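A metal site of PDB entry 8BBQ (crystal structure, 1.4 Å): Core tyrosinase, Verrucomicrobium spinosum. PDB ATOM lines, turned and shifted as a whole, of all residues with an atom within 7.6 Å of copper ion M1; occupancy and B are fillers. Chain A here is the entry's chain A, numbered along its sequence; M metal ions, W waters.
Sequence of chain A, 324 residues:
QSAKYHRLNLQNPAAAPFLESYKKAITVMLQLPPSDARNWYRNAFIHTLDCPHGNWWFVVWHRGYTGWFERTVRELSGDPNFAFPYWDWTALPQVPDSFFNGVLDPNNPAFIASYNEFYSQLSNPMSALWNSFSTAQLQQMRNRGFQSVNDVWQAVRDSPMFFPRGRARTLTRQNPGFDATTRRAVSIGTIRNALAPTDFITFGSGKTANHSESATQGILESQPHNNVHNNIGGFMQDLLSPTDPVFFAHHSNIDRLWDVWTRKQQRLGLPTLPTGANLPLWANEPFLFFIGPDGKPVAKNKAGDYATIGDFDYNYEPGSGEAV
OD1 of Asn 226 lies within hydrogen-bond range of ND1 of His 225.
The backbone carbonyl oxygen (O) of Met 236 sits at hydrogen-bond distance from a ring nitrogen (ND1) of His 229.
The backbone carbonyl oxygen (O) of His 225 lies within hydrogen-bond range of a ring nitrogen (NE2) of His 250, at 3.3 Å.
Residues that only touch copper ion M1: Phe 247 (3.5 Å) and His 250 (3.9 Å).
Of the 15 residues printed, 5 come within 4 Å of copper ion M1.
The nearest printed residue that does not touch copper ion M1 is His 62 (4.3 Å).
Copper ion M1 is bound by a ring nitrogen (NE2) of His 229, a ring nitrogen (NE2) of His 251, a ring nitrogen (NE2) of His 225 and water W1.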
ATOM      1  N   HIS A  47     -22.856  15.815 -35.097  1.00  0.00           N
ATOM      2  CA  HIS A  47     -23.048  14.493 -34.434  1.00  0.00           C
ATOM      3  C   HIS A  47     -23.660  13.506 -35.444  1.00  0.00           C
ATOM      4  O   HIS A  47     -23.147  12.391 -35.628  1.00  0.00           O
ATOM      5  CB  HIS A  47     -23.886  14.673 -33.178  1.00  0.00           C
ATOM      6  CG  HIS A  47     -24.094  13.427 -32.394  1.00  0.00           C
ATOM      7  ND1 HIS A  47     -25.113  12.565 -32.645  1.00  0.00           N
ATOM      8  CD2 HIS A  47     -23.409  12.915 -31.332  1.00  0.00           C
ATOM      9  CE1 HIS A  47     -25.060  11.555 -31.765  1.00  0.00           C
ATOM     10  NE2 HIS A  47     -24.014  11.736 -31.002  1.00  0.00           N
ATOM     11  N   HIS A  53     -20.353   5.536 -32.974  1.00  0.00           N
ATOM     12  CA  HIS A  53     -21.062   4.731 -31.951  1.00  0.00           C
ATOM     13  C   HIS A  53     -20.583   3.274 -32.093  1.00  0.00           C
ATOM     14  O   HIS A  53     -20.338   2.788 -33.220  1.00  0.00           O
ATOM     15  CB  HIS A  53     -22.556   5.163 -31.962  1.00  0.00           C
ATOM     16  CG  HIS A  53     -22.706   6.664 -31.833  1.00  0.00           C
ATOM     17  ND1 HIS A  53     -22.760   7.489 -32.962  1.00  0.00           N
ATOM     18  CD2 HIS A  53     -22.713   7.496 -30.755  1.00  0.00           C
ATOM     19  CE1 HIS A  53     -22.810   8.789 -32.573  1.00  0.00           C
ATOM     20  NE2 HIS A  53     -22.804   8.816 -31.205  1.00  0.00           N
ATOM     21  N   PHE A  58     -15.326   6.274 -29.499  1.00  0.00           N
ATOM     22  CA  PHE A  58     -16.470   6.806 -28.706  1.00  0.00           C
ATOM     23  C   PHE A  58     -16.049   7.945 -27.762  1.00  0.00           C
ATOM     24  O   PHE A  58     -16.455   9.097 -27.939  1.00  0.00           O
ATOM     25  CB  PHE A  58     -17.167   5.647 -27.974  1.00  0.00           C
ATOM     26  CG  PHE A  58     -18.134   6.099 -26.914  1.00  0.00           C
ATOM     27  CD1 PHE A  58     -19.273   6.801 -27.273  1.00  0.00           C
ATOM     28  CD2 PHE A  58     -17.917   5.792 -25.579  1.00  0.00           C
ATOM     29  CE1 PHE A  58     -20.160   7.231 -26.300  1.00  0.00           C
ATOM     30  CE2 PHE A  58     -18.810   6.232 -24.598  1.00  0.00           C
ATOM     31  CZ  PHE A  58     -19.921   6.957 -24.977  1.00  0.00           C
ATOM     32  N   HIS A  62     -16.183  12.278 -28.572  1.00  0.00           N
ATOM     33  CA  HIS A  62     -17.122  13.057 -27.718  1.00  0.00           C
ATOM     34  C   HIS A  62     -16.357  14.096 -26.910  1.00  0.00           C
ATOM     35  O   HIS A  62     -16.921  15.183 -26.628  1.00  0.00           O
ATOM     36  CB  HIS A  62     -18.026  12.142 -26.861  1.00  0.00           C
ATOM     37  CG  HIS A  62     -19.141  11.545 -27.696  1.00  0.00           C
ATOM     38  ND1 HIS A  62     -19.059  10.304 -28.289  1.00  0.00           N
ATOM     39  CD2 HIS A  62     -20.338  12.055 -28.097  1.00  0.00           C
ATOM     40  CE1 HIS A  62     -20.179  10.053 -28.971  1.00  0.00           C
ATOM     41  NE2 HIS A  62     -20.985  11.122 -28.871  1.00  0.00           N
ATOM     42  N   HIS A 225     -24.345   5.115 -20.878  1.00  0.00           N
ATOM     43  CA  HIS A 225     -24.437   6.044 -22.030  1.00  0.00           C
ATOM     44  C   HIS A 225     -25.690   5.729 -22.849  1.00  0.00           C
ATOM     45  O   HIS A 225     -26.514   6.642 -23.024  1.00  0.00           O
ATOM     46  CB  HIS A 225     -23.181   6.024 -22.891  1.00  0.00           C
ATOM     47  CG  HIS A 225     -23.359   6.865 -24.114  1.00  0.00           C
ATOM     48  ND1 HIS A 225     -23.649   6.321 -25.348  1.00  0.00           N
ATOM     49  CD2 HIS A 225     -23.349   8.216 -24.255  1.00  0.00           C
ATOM     50  CE1 HIS A 225     -23.778   7.305 -26.217  1.00  0.00           C
ATOM     51  NE2 HIS A 225     -23.624   8.496 -25.563  1.00  0.00           N
ATOM     52  N   ASN A 226     -25.792   4.532 -23.404  1.00  0.00           N
ATOM     53  CA  ASN A 226     -26.873   4.154 -24.364  1.00  0.00           C
ATOM     54  C   ASN A 226     -28.220   4.163 -23.612  1.00  0.00           C
ATOM     55  O   ASN A 226     -29.214   4.656 -24.150  1.00  0.00           O
ATOM     56  CB  ASN A 226     -26.558   2.833 -25.081  1.00  0.00           C
ATOM     57  CG  ASN A 226     -25.418   2.926 -26.103  1.00  0.00           C
ATOM     58  OD1 ASN A 226     -24.905   4.010 -26.385  1.00  0.00           O
ATOM     59  ND2 ASN A 226     -24.992   1.773 -26.640  1.00  0.00           N
ATOM     60  N   HIS A 229     -29.616   7.692 -22.890  1.00  0.00           N
ATOM     61  CA  HIS A 229     -30.080   8.228 -24.192  1.00  0.00           C
ATOM     62  C   HIS A 229     -31.517   7.740 -24.449  1.00  0.00           C
ATOM     63  O   HIS A 229     -32.448   8.559 -24.690  1.00  0.00           O
ATOM     64  CB  HIS A 229     -29.138   7.819 -25.327  1.00  0.00           C
ATOM     65  CG  HIS A 229     -28.090   8.840 -25.643  1.00  0.00           C
ATOM     66  ND1 HIS A 229     -28.349   9.967 -26.399  1.00  0.00           N
ATOM     67  CD2 HIS A 229     -26.775   8.899 -25.315  1.00  0.00           C
ATOM     68  CE1 HIS A 229     -27.220  10.659 -26.535  1.00  0.00           C
ATOM     69  NE2 HIS A 229     -26.272  10.062 -25.860  1.00  0.00           N
ATOM     70  N   MET A 236     -33.019  12.509 -27.852  1.00  0.00           N
ATOM     71  CA  MET A 236     -31.884  11.835 -27.200  1.00  0.00           C
ATOM     72  C   MET A 236     -31.807  10.367 -27.646  1.00  0.00           C
ATOM     73  O   MET A 236     -30.775   9.778 -27.403  1.00  0.00           O
ATOM     74  CB  MET A 236     -31.936  11.967 -25.668  1.00  0.00           C
ATOM     75  CG  MET A 236     -31.480  13.333 -25.218  1.00  0.00           C
ATOM     76  SD  MET A 236     -29.670  13.557 -25.416  1.00  0.00           S
ATOM     77  CE  MET A 236     -29.029  12.576 -24.080  1.00  0.00           C
ATOM     78  N   ASP A 238     -31.758   9.198 -30.705  1.00  0.00           N
ATOM     79  CA  ASP A 238     -31.207   9.030 -32.076  1.00  0.00           C
ATOM     80  C   ASP A 238     -30.168  10.107 -32.381  1.00  0.00           C
ATOM     81  O   ASP A 238     -29.756  10.850 -31.446  1.00  0.00           O
ATOM     82  CB  ASP A 238     -32.363   8.929 -33.081  1.00  0.00           C
ATOM     83  CG  ASP A 238     -32.091   7.919 -34.193  1.00  0.00           C
ATOM     84  OD1 ASP A 238     -30.975   7.933 -34.748  1.00  0.00           O
ATOM     85  OD2 ASP A 238     -33.019   7.124 -34.483  1.00  0.00           O
ATOM     86  N   SER A 241     -29.527  13.784 -31.258  1.00  0.00           N
ATOM     87  CA  SER A 241     -29.511  13.915 -29.773  1.00  0.00           C
ATOM     88  C   SER A 241     -28.972  15.265 -29.276  1.00  0.00           C
ATOM     89  O   SER A 241     -29.533  15.758 -28.304  1.00  0.00           O
ATOM     90  CB  SER A 241     -28.807  12.765 -29.119  1.00  0.00           C
ATOM     91  OG  SER A 241     -27.541  12.477 -29.705  1.00  0.00           O
ATOM     92  N   PRO A 242     -27.919  15.916 -29.865  1.00  0.00           N
ATOM     93  CA  PRO A 242     -27.462  17.210 -29.361  1.00  0.00           C
ATOM     94  C   PRO A 242     -28.457  18.364 -29.533  1.00  0.00           C
ATOM     95  O   PRO A 242     -28.206  19.439 -29.025  1.00  0.00           O
ATOM     96  CB  PRO A 242     -26.165  17.516 -30.109  1.00  0.00           C
ATOM     97  CG  PRO A 242     -25.732  16.131 -30.650  1.00  0.00           C
ATOM     98  CD  PRO A 242     -27.043  15.408 -30.939  1.00  0.00           C
ATOM     99  N   PHE A 247     -27.906  16.784 -23.617  1.00  0.00           N
ATOM    100  CA  PHE A 247     -26.854  15.992 -24.300  1.00  0.00           C
ATOM    101  C   PHE A 247     -25.482  16.390 -23.749  1.00  0.00           C
ATOM    102  O   PHE A 247     -24.696  15.508 -23.412  1.00  0.00           O
ATOM    103  CB  PHE A 247     -26.885  16.202 -25.812  1.00  0.00           C
ATOM    104  CG  PHE A 247     -25.771  15.486 -26.532  1.00  0.00           C
ATOM    105  CD1 PHE A 247     -24.534  16.067 -26.708  1.00  0.00           C
ATOM    106  CD2 PHE A 247     -25.981  14.220 -27.031  1.00  0.00           C
ATOM    107  CE1 PHE A 247     -23.535  15.404 -27.407  1.00  0.00           C
ATOM    108  CE2 PHE A 247     -24.989  13.554 -27.719  1.00  0.00           C
ATOM    109  CZ  PHE A 247     -23.774  14.160 -27.932  1.00  0.00           C
ATOM    110  N   HIS A 250     -24.923  15.259 -20.121  1.00  0.00           N
ATOM    111  CA  HIS A 250     -24.712  13.796 -20.225  1.00  0.00           C
ATOM    112  C   HIS A 250     -23.264  13.544 -20.623  1.00  0.00           C
ATOM    113  O   HIS A 250     -22.568  12.762 -19.935  1.00  0.00           O
ATOM    114  CB  HIS A 250     -25.729  13.192 -21.216  1.00  0.00           C
ATOM    115  CG  HIS A 250     -25.613  11.722 -21.436  1.00  0.00           C
ATOM    116  ND1 HIS A 250     -25.551  10.844 -20.400  1.00  0.00           N
ATOM    117  CD2 HIS A 250     -25.637  10.984 -22.570  1.00  0.00           C
ATOM    118  CE1 HIS A 250     -25.507   9.611 -20.880  1.00  0.00           C
ATOM    119  NE2 HIS A 250     -25.562   9.651 -22.206  1.00  0.00           N
ATOM    120  N   HIS A 251     -22.778  14.227 -21.665  1.00  0.00           N
ATOM    121  CA  HIS A 251     -21.408  13.957 -22.192  1.00  0.00           C
ATOM    122  C   HIS A 251     -20.328  14.568 -21.314  1.00  0.00           C
ATOM    123  O   HIS A 251     -19.200  14.017 -21.273  1.00  0.00           O
ATOM    124  CB  HIS A 251     -21.292  14.331 -23.671  1.00  0.00           C
ATOM    125  CG  HIS A 251     -21.713  13.163 -24.475  1.00  0.00           C
ATOM    126  ND1 HIS A 251     -20.889  12.053 -24.701  1.00  0.00           N
ATOM    127  CD2 HIS A 251     -22.930  12.821 -24.937  1.00  0.00           C
ATOM    128  CE1 HIS A 251     -21.592  11.113 -25.317  1.00  0.00           C
ATOM    129  NE2 HIS A 251     -22.809  11.597 -25.522  1.00  0.00           N
ATOM    130  N   ILE A 254     -19.938  11.661 -18.982  1.00  0.00           N
ATOM    131  CA  ILE A 254     -19.177  10.571 -19.655  1.00  0.00           C
ATOM    132  C   ILE A 254     -17.688  10.938 -19.676  1.00  0.00           C
ATOM    133  O   ILE A 254     -16.853  10.126 -19.352  1.00  0.00           O
ATOM    134  CB  ILE A 254     -19.724  10.304 -21.052  1.00  0.00           C
ATOM    135  CG1 ILE A 254     -21.163   9.731 -21.022  1.00  0.00           C
ATOM    136  CG2 ILE A 254     -18.764   9.464 -21.888  1.00  0.00           C
ATOM    137  CD1 ILE A 254     -21.265   8.345 -20.486  1.00  0.00           C
HETATM  138 CU    CU M   1     -24.325  10.418 -26.196  1.00  0.00          CU
HETATM  139 CU    CU M   2     -22.802  10.446 -29.841  1.00  0.00          CU
HETATM  140  O   HOH W   1     -24.200  10.016 -28.399  1.00  0.00           O
